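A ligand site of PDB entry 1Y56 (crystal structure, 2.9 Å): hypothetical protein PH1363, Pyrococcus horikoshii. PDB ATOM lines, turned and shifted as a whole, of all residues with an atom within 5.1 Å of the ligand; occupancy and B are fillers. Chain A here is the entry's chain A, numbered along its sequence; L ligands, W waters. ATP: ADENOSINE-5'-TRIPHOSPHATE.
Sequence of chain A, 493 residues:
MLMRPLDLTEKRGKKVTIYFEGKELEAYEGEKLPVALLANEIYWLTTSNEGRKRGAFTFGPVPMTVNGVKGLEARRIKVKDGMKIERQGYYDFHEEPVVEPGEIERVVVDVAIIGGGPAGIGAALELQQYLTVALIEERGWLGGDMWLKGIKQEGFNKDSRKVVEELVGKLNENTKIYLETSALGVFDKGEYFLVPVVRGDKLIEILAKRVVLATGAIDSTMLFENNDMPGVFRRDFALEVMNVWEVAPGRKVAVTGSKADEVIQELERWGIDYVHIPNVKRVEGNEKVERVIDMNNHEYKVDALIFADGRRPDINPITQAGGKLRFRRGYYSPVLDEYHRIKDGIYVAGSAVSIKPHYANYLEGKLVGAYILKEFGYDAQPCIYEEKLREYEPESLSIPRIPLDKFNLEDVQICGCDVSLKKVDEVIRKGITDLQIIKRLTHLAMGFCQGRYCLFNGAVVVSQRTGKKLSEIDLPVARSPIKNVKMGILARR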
ATOM      1  N   ILE A 114     -26.197  -2.240  -3.929  1.00  0.00           N
ATOM      2  CA  ILE A 114     -26.594  -0.971  -4.538  1.00  0.00           C
ATOM      3  C   ILE A 114     -25.729   0.158  -4.008  1.00  0.00           C
ATOM      4  O   ILE A 114     -25.819   0.546  -2.836  1.00  0.00           O
ATOM      5  CB  ILE A 114     -28.065  -0.639  -4.292  1.00  0.00           C
ATOM      6  CG1 ILE A 114     -28.956  -1.782  -4.794  1.00  0.00           C
ATOM      7  CG2 ILE A 114     -28.425   0.723  -4.943  1.00  0.00           C
ATOM      8  CD1 ILE A 114     -30.406  -1.632  -4.426  1.00  0.00           C
ATOM      9  N   GLY A 115     -24.900   0.693  -4.898  1.00  0.00           N
ATOM     10  CA  GLY A 115     -24.016   1.777  -4.554  1.00  0.00           C
ATOM     11  C   GLY A 115     -22.592   1.311  -4.628  1.00  0.00           C
ATOM     12  O   GLY A 115     -22.239   0.331  -3.995  1.00  0.00           O
ATOM     13  N   GLY A 116     -21.756   2.030  -5.390  1.00  0.00           N
ATOM     14  CA  GLY A 116     -20.376   1.605  -5.654  1.00  0.00           C
ATOM     15  C   GLY A 116     -19.268   2.432  -5.025  1.00  0.00           C
ATOM     16  O   GLY A 116     -18.168   2.482  -5.548  1.00  0.00           O
ATOM     17  N   GLY A 117     -19.549   3.085  -3.895  1.00  0.00           N
ATOM     18  CA  GLY A 117     -18.495   3.784  -3.157  1.00  0.00           C
ATOM     19  C   GLY A 117     -17.687   2.791  -2.345  1.00  0.00           C
ATOM     20  O   GLY A 117     -17.813   1.567  -2.536  1.00  0.00           O
ATOM     21  N   PRO A 118     -16.838   3.300  -1.428  1.00  0.00           N
ATOM     22  CA  PRO A 118     -16.031   2.432  -0.549  1.00  0.00           C
ATOM     23  C   PRO A 118     -16.856   1.347   0.169  1.00  0.00           C
ATOM     24  O   PRO A 118     -16.365   0.227   0.338  1.00  0.00           O
ATOM     25  CB  PRO A 118     -15.429   3.405   0.467  1.00  0.00           C
ATOM     26  CG  PRO A 118     -16.143   4.735   0.244  1.00  0.00           C
ATOM     27  CD  PRO A 118     -16.584   4.736  -1.171  1.00  0.00           C
ATOM     28  N   ALA A 119     -18.081   1.678   0.590  1.00  0.00           N
ATOM     29  CA  ALA A 119     -18.933   0.696   1.252  1.00  0.00           C
ATOM     30  C   ALA A 119     -19.246  -0.448   0.304  1.00  0.00           C
ATOM     31  O   ALA A 119     -19.028  -1.624   0.640  1.00  0.00           O
ATOM     32  CB  ALA A 119     -20.214   1.329   1.747  1.00  0.00           C
ATOM     33  N   GLY A 120     -19.754  -0.110  -0.885  1.00  0.00           N
ATOM     34  CA  GLY A 120     -20.111  -1.100  -1.887  1.00  0.00           C
ATOM     35  C   GLY A 120     -18.952  -1.987  -2.289  1.00  0.00           C
ATOM     36  O   GLY A 120     -19.063  -3.209  -2.288  1.00  0.00           O
ATOM     37  N   ILE A 136     -23.872  -2.376  -8.257  1.00  0.00           N
ATOM     38  CA  ILE A 136     -24.651  -1.445  -9.054  1.00  0.00           C
ATOM     39  C   ILE A 136     -24.243  -0.010  -8.717  1.00  0.00           C
ATOM     40  O   ILE A 136     -24.222   0.364  -7.546  1.00  0.00           O
ATOM     41  CB  ILE A 136     -26.149  -1.650  -8.802  1.00  0.00           C
ATOM     42  CG1 ILE A 136     -26.554  -3.093  -9.112  1.00  0.00           C
ATOM     43  CG2 ILE A 136     -26.988  -0.688  -9.620  1.00  0.00           C
ATOM     44  CD1 ILE A 136     -27.808  -3.534  -8.393  1.00  0.00           C
ATOM     45  N   GLU A 137     -23.917   0.779  -9.746  1.00  0.00           N
ATOM     46  CA  GLU A 137     -23.574   2.192  -9.566  1.00  0.00           C
ATOM     47  C   GLU A 137     -24.048   3.027 -10.742  1.00  0.00           C
ATOM     48  O   GLU A 137     -23.745   2.725 -11.896  1.00  0.00           O
ATOM     49  CB  GLU A 137     -22.060   2.342  -9.405  1.00  0.00           C
ATOM     50  CG  GLU A 137     -21.548   3.770  -9.438  1.00  0.00           C
ATOM     51  CD  GLU A 137     -21.912   4.579  -8.200  1.00  0.00           C
ATOM     52  OE1 GLU A 137     -21.401   4.300  -7.098  1.00  0.00           O
ATOM     53  OE2 GLU A 137     -22.716   5.524  -8.329  1.00  0.00           O
ATOM     54  N   GLU A 138     -24.790   4.096 -10.447  1.00  0.00           N
ATOM     55  CA  GLU A 138     -25.301   4.937 -11.536  1.00  0.00           C
ATOM     56  C   GLU A 138     -24.247   5.879 -12.098  1.00  0.00           C
ATOM     57  O   GLU A 138     -24.469   6.522 -13.114  1.00  0.00           O
ATOM     58  CB  GLU A 138     -26.533   5.710 -11.094  1.00  0.00           C
ATOM     59  CG  GLU A 138     -26.263   6.935 -10.235  1.00  0.00           C
ATOM     60  CD  GLU A 138     -27.551   7.571  -9.694  1.00  0.00           C
ATOM     61  OE1 GLU A 138     -27.560   7.919  -8.475  1.00  0.00           O
ATOM     62  OE2 GLU A 138     -28.552   7.704 -10.477  1.00  0.00           O
ATOM     63  N   ARG A 139     -23.082   5.918 -11.452  1.00  0.00           N
ATOM     64  CA  ARG A 139     -22.204   7.049 -11.583  1.00  0.00           C
ATOM     65  C   ARG A 139     -21.185   7.005 -12.712  1.00  0.00           C
ATOM     66  O   ARG A 139     -20.568   8.026 -12.989  1.00  0.00           O
ATOM     67  CB  ARG A 139     -21.484   7.309 -10.266  1.00  0.00           C
ATOM     68  CG  ARG A 139     -21.139   8.737 -10.023  1.00  0.00           C
ATOM     69  CD  ARG A 139     -22.042   9.324  -8.995  1.00  0.00           C
ATOM     70  NE  ARG A 139     -21.497   9.131  -7.655  1.00  0.00           N
ATOM     71  CZ  ARG A 139     -21.094  10.116  -6.860  1.00  0.00           C
ATOM     72  NH1 ARG A 139     -21.164  11.384  -7.244  1.00  0.00           N
ATOM     73  NH2 ARG A 139     -20.634   9.836  -5.642  1.00  0.00           N
ATOM     74  N   GLY A 143     -15.338   4.717  -7.874  1.00  0.00           N
ATOM     75  CA  GLY A 143     -14.994   5.207  -6.532  1.00  0.00           C
ATOM     76  C   GLY A 143     -16.287   5.554  -5.832  1.00  0.00           C
ATOM     77  O   GLY A 143     -17.369   5.178  -6.306  1.00  0.00           O
ATOM     78  N   GLY A 144     -16.257   6.293  -4.745  1.00  0.00           N
ATOM     79  CA  GLY A 144     -17.534   6.819  -4.298  1.00  0.00           C
ATOM     80  C   GLY A 144     -17.562   8.309  -4.389  1.00  0.00           C
ATOM     81  O   GLY A 144     -17.269   8.901  -5.422  1.00  0.00           O
ATOM     82  N   ASP A 145     -17.902   8.924  -3.264  1.00  0.00           N
ATOM     83  CA  ASP A 145     -17.558  10.287  -3.017  1.00  0.00           C
ATOM     84  C   ASP A 145     -16.031  10.403  -2.941  1.00  0.00           C
ATOM     85  O   ASP A 145     -15.465  11.483  -3.062  1.00  0.00           O
ATOM     86  CB  ASP A 145     -18.153  10.707  -1.693  1.00  0.00           C
ATOM     87  CG  ASP A 145     -17.967  12.155  -1.419  1.00  0.00           C
ATOM     88  OD1 ASP A 145     -17.071  12.502  -0.629  1.00  0.00           O
ATOM     89  OD2 ASP A 145     -18.708  12.961  -2.012  1.00  0.00           O
ATOM     90  N   MET A 146     -15.362   9.278  -2.741  1.00  0.00           N
ATOM     91  CA  MET A 146     -13.934   9.228  -2.534  1.00  0.00           C
ATOM     92  C   MET A 146     -13.177   9.624  -3.793  1.00  0.00           C
ATOM     93  O   MET A 146     -12.117  10.259  -3.721  1.00  0.00           O
ATOM     94  CB  MET A 146     -13.563   7.815  -2.129  1.00  0.00           C
ATOM     95  CG  MET A 146     -12.343   7.714  -1.278  1.00  0.00           C
ATOM     96  SD  MET A 146     -12.225   6.053  -0.594  1.00  0.00           S
ATOM     97  CE  MET A 146     -10.443   5.990  -0.392  1.00  0.00           C
ATOM     98  N   THR A 181     -25.537   2.806 -14.036  1.00  0.00           N
ATOM     99  CA  THR A 181     -26.702   1.978 -13.814  1.00  0.00           C
ATOM    100  C   THR A 181     -27.542   2.414 -12.601  1.00  0.00           C
ATOM    101  O   THR A 181     -27.075   2.373 -11.475  1.00  0.00           O
ATOM    102  CB  THR A 181     -26.317   0.510 -13.642  1.00  0.00           C
ATOM    103  OG1 THR A 181     -25.630   0.045 -14.818  1.00  0.00           O
ATOM    104  CG2 THR A 181     -27.538  -0.336 -13.405  1.00  0.00           C
ATOM    105  N   SER A 182     -28.789   2.808 -12.864  1.00  0.00           N
ATOM    106  CA  SER A 182     -29.723   3.259 -11.829  1.00  0.00           C
ATOM    107  C   SER A 182     -30.630   2.146 -11.319  1.00  0.00           C
ATOM    108  O   SER A 182     -31.411   1.592 -12.094  1.00  0.00           O
ATOM    109  CB  SER A 182     -30.579   4.406 -12.360  1.00  0.00           C
ATOM    110  OG  SER A 182     -29.844   5.617 -12.392  1.00  0.00           O
ATOM    111  N   ALA A 183     -30.522   1.842 -10.034  1.00  0.00           N
ATOM    112  CA  ALA A 183     -31.468   0.929  -9.386  1.00  0.00           C
ATOM    113  C   ALA A 183     -32.781   1.652  -9.091  1.00  0.00           C
ATOM    114  O   ALA A 183     -32.784   2.784  -8.580  1.00  0.00           O
ATOM    115  CB  ALA A 183     -30.885   0.357  -8.112  1.00  0.00           C
ATOM    116  N   ALA A 214     -25.626   0.217  -0.135  1.00  0.00           N
ATOM    117  CA  ALA A 214     -24.367   0.928   0.095  1.00  0.00           C
ATOM    118  C   ALA A 214     -24.509   2.250  -0.636  1.00  0.00           C
ATOM    119  O   ALA A 214     -23.766   2.573  -1.589  1.00  0.00           O
ATOM    120  CB  ALA A 214     -23.195   0.125  -0.410  1.00  0.00           C
ATOM    121  N   THR A 215     -25.477   3.015  -0.171  1.00  0.00           N
ATOM    122  CA  THR A 215     -26.240   3.904  -1.027  1.00  0.00           C
ATOM    123  C   THR A 215     -25.731   5.333  -0.933  1.00  0.00           C
ATOM    124  O   THR A 215     -25.927   6.132  -1.845  1.00  0.00           O
ATOM    125  CB  THR A 215     -27.747   3.730  -0.706  1.00  0.00           C
ATOM    126  OG1 THR A 215     -28.465   3.637  -1.927  1.00  0.00           O
ATOM    127  CG2 THR A 215     -28.306   4.841   0.250  1.00  0.00           C
ATOM    128  N   GLY A 216     -25.051   5.645   0.173  1.00  0.00           N
ATOM    129  CA  GLY A 216     -24.379   6.913   0.350  1.00  0.00           C
ATOM    130  C   GLY A 216     -25.169   7.985   1.059  1.00  0.00           C
ATOM    131  O   GLY A 216     -26.370   7.819   1.372  1.00  0.00           O
ATOM    132  N   ALA A 217     -24.474   9.085   1.324  1.00  0.00           N
ATOM    133  CA  ALA A 217     -25.050  10.309   1.840  1.00  0.00           C
ATOM    134  C   ALA A 217     -25.103  11.325   0.704  1.00  0.00           C
ATOM    135  O   ALA A 217     -24.371  11.207  -0.269  1.00  0.00           O
ATOM    136  CB  ALA A 217     -24.193  10.855   2.976  1.00  0.00           C
ATOM    137  N   ARG A 311     -22.776  16.339   4.592  1.00  0.00           N
ATOM    138  CA  ARG A 311     -23.582  15.307   3.944  1.00  0.00           C
ATOM    139  C   ARG A 311     -24.482  14.613   4.965  1.00  0.00           C
ATOM    140  O   ARG A 311     -24.154  14.543   6.156  1.00  0.00           O
ATOM    141  CB  ARG A 311     -22.683  14.271   3.264  1.00  0.00           C
ATOM    142  CG  ARG A 311     -21.410  14.825   2.652  1.00  0.00           C
ATOM    143  CD  ARG A 311     -21.044  14.039   1.420  1.00  0.00           C
ATOM    144  NE  ARG A 311     -20.545  12.693   1.706  1.00  0.00           N
ATOM    145  CZ  ARG A 311     -20.797  11.609   0.977  1.00  0.00           C
ATOM    146  NH1 ARG A 311     -20.278  10.449   1.308  1.00  0.00           N
ATOM    147  NH2 ARG A 311     -21.604  11.672  -0.078  1.00  0.00           N
ATOM    148  N   ASP A 314     -28.633   9.477   2.418  1.00  0.00           N
ATOM    149  CA  ASP A 314     -29.763   9.461   1.500  1.00  0.00           C
ATOM    150  C   ASP A 314     -30.746   8.412   2.038  1.00  0.00           C
ATOM    151  O   ASP A 314     -30.435   7.223   2.071  1.00  0.00           O
ATOM    152  CB  ASP A 314     -29.281   9.126   0.080  1.00  0.00           C
ATOM    153  CG  ASP A 314     -30.387   9.207  -0.952  1.00  0.00           C
ATOM    154  OD1 ASP A 314     -31.540   9.569  -0.619  1.00  0.00           O
ATOM    155  OD2 ASP A 314     -30.100   8.891  -2.130  1.00  0.00           O
ATOM    156  N   ALA A 349     -24.979  -0.377   4.613  1.00  0.00           N
ATOM    157  CA  ALA A 349     -23.575  -0.066   4.960  1.00  0.00           C
ATOM    158  C   ALA A 349     -23.055   1.230   4.345  1.00  0.00           C
ATOM    159  O   ALA A 349     -23.421   1.601   3.225  1.00  0.00           O
ATOM    160  CB  ALA A 349     -22.656  -1.229   4.596  1.00  0.00           C
ATOM    161  N   GLY A 350     -22.185   1.912   5.104  1.00  0.00           N
ATOM    162  CA  GLY A 350     -21.527   3.130   4.644  1.00  0.00           C
ATOM    163  C   GLY A 350     -22.067   4.437   5.204  1.00  0.00           C
ATOM    164  O   GLY A 350     -22.507   4.507   6.362  1.00  0.00           O
ATOM    165  N   SER A 351     -22.038   5.478   4.386  1.00  0.00           N
ATOM    166  CA  SER A 351     -22.533   6.790   4.779  1.00  0.00           C
ATOM    167  C   SER A 351     -24.051   6.837   4.655  1.00  0.00           C
ATOM    168  O   SER A 351     -24.678   7.856   4.953  1.00  0.00           O
ATOM    169  CB  SER A 351     -21.912   7.858   3.907  1.00  0.00           C
ATOM    170  OG  SER A 351     -22.252   7.641   2.549  1.00  0.00           O
ATOM    171  N   ALA A 352     -24.622   5.728   4.197  1.00  0.00           N
ATOM    172  CA  ALA A 352     -26.058   5.499   4.286  1.00  0.00           C
ATOM    173  C   ALA A 352     -26.443   5.245   5.734  1.00  0.00           C
ATOM    174  O   ALA A 352     -27.567   5.528   6.129  1.00  0.00           O
ATOM    175  CB  ALA A 352     -26.461   4.328   3.413  1.00  0.00           C
ATOM    176  N   LYS A 356     -19.088   9.377   8.638  1.00  0.00           N
ATOM    177  CA  LYS A 356     -17.802   8.961   9.202  1.00  0.00           C
ATOM    178  C   LYS A 356     -16.773   8.836   8.070  1.00  0.00           C
ATOM    179  O   LYS A 356     -17.176   8.837   6.896  1.00  0.00           O
ATOM    180  CB  LYS A 356     -17.930   7.655  10.011  1.00  0.00           C
ATOM    181  CG  LYS A 356     -18.502   6.458   9.244  1.00  0.00           C
ATOM    182  CD  LYS A 356     -19.033   5.395  10.197  1.00  0.00           C
ATOM    183  CE  LYS A 356     -19.695   4.212   9.466  1.00  0.00           C
ATOM    184  NZ  LYS A 356     -20.985   4.547   8.774  1.00  0.00           N
ATOM    185  N   PRO A 357     -15.467   8.749   8.397  1.00  0.00           N
ATOM    186  CA  PRO A 357     -14.419   8.686   7.371  1.00  0.00           C
ATOM    187  C   PRO A 357     -14.613   7.565   6.335  1.00  0.00           C
ATOM    188  O   PRO A 357     -15.238   6.551   6.645  1.00  0.00           O
ATOM    189  CB  PRO A 357     -13.154   8.411   8.195  1.00  0.00           C
ATOM    190  CG  PRO A 357     -13.448   8.957   9.487  1.00  0.00           C
ATOM    191  CD  PRO A 357     -14.889   8.702   9.740  1.00  0.00           C
ATOM    192  N   HIS A 358     -14.069   7.747   5.130  1.00  0.00           N
ATOM    193  CA  HIS A 358     -14.195   6.762   4.054  1.00  0.00           C
ATOM    194  C   HIS A 358     -13.798   5.380   4.525  1.00  0.00           C
ATOM    195  O   HIS A 358     -14.505   4.411   4.293  1.00  0.00           O
ATOM    196  CB  HIS A 358     -13.326   7.132   2.865  1.00  0.00           C
ATOM    197  CG  HIS A 358     -13.730   8.394   2.195  1.00  0.00           C
ATOM    198  ND1 HIS A 358     -14.956   8.553   1.585  1.00  0.00           N
ATOM    199  CD2 HIS A 358     -13.074   9.575   2.036  1.00  0.00           C
ATOM    200  CE1 HIS A 358     -15.047   9.776   1.078  1.00  0.00           C
ATOM    201  NE2 HIS A 358     -13.913  10.414   1.344  1.00  0.00           N
ATOM    202  N   ASN A 361     -16.474   3.532   6.395  1.00  0.00           N
ATOM    203  CA  ASN A 361     -17.575   3.077   5.557  1.00  0.00           C
ATOM    204  C   ASN A 361     -17.136   1.856   4.751  1.00  0.00           C
ATOM    205  O   ASN A 361     -17.937   0.946   4.495  1.00  0.00           O
ATOM    206  CB  ASN A 361     -18.077   4.210   4.651  1.00  0.00           C
ATOM    207  CG  ASN A 361     -18.646   5.385   5.449  1.00  0.00           C
ATOM    208  OD1 ASN A 361     -19.328   5.193   6.465  1.00  0.00           O
ATOM    209  ND2 ASN A 361     -18.352   6.604   5.006  1.00  0.00           N
ATOM    210  N   ILE A 482     -37.215   4.797  -7.081  1.00  0.00           N
ATOM    211  CA  ILE A 482     -36.433   5.725  -6.261  1.00  0.00           C
ATOM    212  C   ILE A 482     -35.605   6.669  -7.140  1.00  0.00           C
ATOM    213  O   ILE A 482     -35.211   7.757  -6.707  1.00  0.00           O
ATOM    214  CB  ILE A 482     -35.555   5.021  -5.185  1.00  0.00           C
ATOM    215  CG1 ILE A 482     -34.556   4.044  -5.805  1.00  0.00           C
ATOM    216  CG2 ILE A 482     -36.448   4.343  -4.159  1.00  0.00           C
ATOM    217  CD1 ILE A 482     -33.414   3.685  -4.875  1.00  0.00           C
ATOM    218  N   LYS A 483     -35.361   6.246  -8.376  1.00  0.00           N
ATOM    219  CA  LYS A 483     -34.728   7.089  -9.369  1.00  0.00           C
ATOM    220  C   LYS A 483     -35.631   7.245 -10.578  1.00  0.00           C
ATOM    221  O   LYS A 483     -36.340   6.311 -10.940  1.00  0.00           O
ATOM    222  CB  LYS A 483     -33.386   6.510  -9.795  1.00  0.00           C
ATOM    223  CG  LYS A 483     -32.319   6.618  -8.731  1.00  0.00           C
ATOM    224  CD  LYS A 483     -31.768   8.031  -8.617  1.00  0.00           C
ATOM    225  CE  LYS A 483     -30.557   8.012  -7.696  1.00  0.00           C
ATOM    226  NZ  LYS A 483     -30.218   9.350  -7.122  1.00  0.00           N
HETATM  227  PG  ATP L   1     -18.381   7.418   1.498  1.00  0.00           P
HETATM  228  O1G ATP L   1     -19.700   8.078   1.746  1.00  0.00           O
HETATM  229  O2G ATP L   1     -17.398   7.580   2.639  1.00  0.00           O
HETATM  230  O3G ATP L   1     -17.752   7.697   0.151  1.00  0.00           O
HETATM  231  PB  ATP L   1     -20.070   5.159   0.856  1.00  0.00           P
HETATM  232  O1B ATP L   1     -20.930   4.737   2.036  1.00  0.00           O
HETATM  233  O2B ATP L   1     -19.636   4.177  -0.196  1.00  0.00           O
HETATM  234  O3B ATP L   1     -18.725   5.832   1.444  1.00  0.00           O
HETATM  235  PA  ATP L   1     -20.692   7.026  -1.263  1.00  0.00           P
HETATM  236  O1A ATP L   1     -19.224   7.154  -1.564  1.00  0.00           O
HETATM  237  O2A ATP L   1     -21.560   8.262  -1.239  1.00  0.00           O
HETATM  238  O3A ATP L   1     -20.917   6.352   0.183  1.00  0.00           O
HETATM  239  O5' ATP L   1     -21.272   5.961  -2.331  1.00  0.00           O
HETATM  240  C5' ATP L   1     -22.665   5.916  -2.629  1.00  0.00           C
HETATM  241  C4' ATP L   1     -22.886   5.553  -4.088  1.00  0.00           C
HETATM  242  O4' ATP L   1     -24.165   4.958  -4.259  1.00  0.00           O
HETATM  243  C3' ATP L   1     -22.885   6.812  -4.934  1.00  0.00           C
HETATM  244  O3' ATP L   1     -21.901   6.605  -5.923  1.00  0.00           O
HETATM  245  C2' ATP L   1     -24.286   6.885  -5.530  1.00  0.00           C
HETATM  246  O2' ATP L   1     -24.300   7.331  -6.893  1.00  0.00           O
HETATM  247  C1' ATP L   1     -24.732   5.442  -5.471  1.00  0.00           C
HETATM  248  N9  ATP L   1     -26.204   5.290  -5.519  1.00  0.00           N
HETATM  249  C8  ATP L   1     -27.112   5.804  -4.676  1.00  0.00           C
HETATM  250  N7  ATP L   1     -28.355   5.436  -5.086  1.00  0.00           N
HETATM  251  C5  ATP L   1     -28.214   4.670  -6.199  1.00  0.00           C
HETATM  252  C6  ATP L   1     -29.109   4.000  -7.034  1.00  0.00           C
HETATM  253  N6  ATP L   1     -30.444   4.043  -6.815  1.00  0.00           N
HETATM  254  N1  ATP L   1     -28.621   3.326  -8.074  1.00  0.00           N
HETATM  255  C2  ATP L   1     -27.303   3.260  -8.328  1.00  0.00           C
HETATM  256  N3  ATP L   1     -26.414   3.882  -7.544  1.00  0.00           N
HETATM  257  C4  ATP L   1     -26.850   4.588  -6.463  1.00  0.00           C
HETATM  258  O   HOH W   1     -21.093   2.439  -1.619  1.00  0.00           O
HETATM  259  O   HOH W   2     -30.574   6.533  -3.805  1.00  0.00           O
HETATM  260  O   HOH W   3     -23.576   3.967   1.934  1.00  0.00           O
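The guanidinium group (NH1) of Arg 311 lies within salt-bridge range of an oxygen (O1G) of the ligand (2.5 Å). OE1 of Glu 137 sits at hydrogen-bond distance from O3' of the ligand (2.6 Å). The backbone NH (N) of Ser 351 lies within hydrogen-bond range of an oxygen (O1B) of the ligand (2.7 Å). An oxygen (O1G) of the ligand sits at hydrogen-bond distance from the side-chain hydroxyl (OG) of Ser 351, 2.7 Å away. ND2 of Asn 361 is in hydrogen-bond range of O2G of the ligand, 2.7 Å away. N of Asp 145 lies within hydrogen-bond range of O1A of the ligand (2.8 Å). O2G of the ligand is in hydrogen-bond range of ND1 of His 358 (2.8 Å). The backbone NH of Ala 119 lies within hydrogen-bond range of an oxygen (O2B) of the ligand (3.0 Å). The guanidinium group of Arg 139 lies within hydrogen-bond range of an oxygen (O3') of the ligand (3.1 Å). N of Ala 183 sits at hydrogen-bond distance from N1 of the ligand, 3.1 Å away. O of Ala 183 lies within hydrogen-bond range of N6 of the ligand, at 3.2 Å. N3 of the ligand lies within hydrogen-bond range of N of Glu 138, at 3.3 Å.
O of Glu 137 lies within hydrogen-bond range of N of Thr 181, 2.8 Å away. OG of Ser 351 sits at hydrogen-bond distance from N of Ala 217. The side-chain amide oxygen (OD1) of Asn 361 sits at hydrogen-bond distance from the side-chain amino group (NZ) of Lys 356 (2.9 Å). The backbone carbonyl oxygen of Gly 144 lies within hydrogen-bond range of the guanidinium group of Arg 139, at 3.5 Å. The backbone carbonyl oxygen (O) of Thr 181 lies within hydrogen-bond range of the backbone NH (N) of Glu 138 (3.0 Å). The side-chain carboxylate of Glu 138 is in salt-bridge range of the side-chain amino group of Lys 483, at 3.3 Å. The backbone carbonyl oxygen (O) of Gly 216 is in hydrogen-bond range of the backbone NH (N) of Asp 314, at 3.0 Å. O of Ile 114 is in hydrogen-bond range of N of Ala 214 (2.7 Å).
An oxygen (O2B) of the ligand lies close to the backbone nitrogen (N) of Pro 118. O4' of the ligand sits close to O of Thr 215, at 3.2 Å. Merely in contact with the ligand: Gly 350, Gly 117, Gly 115, Gly 144, Thr 181, Gly 216, Ile 482, Ala 214, Lys 483, Ser 182, Gly 116, Ile 114 and Ala 217.
Water W1 lies within hydrogen-bond range of O of Ala 214 (2.7 Å), O2B of the ligand (2.7 Å), N of Gly 117 (2.8 Å), N of Gly 120 (3.0 Å) and O of Gly 115 (3.4 Å). Water W2 lies within hydrogen-bond range of N7 of the ligand (2.8 Å) and OD2 of Asp 314 (2.9 Å).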
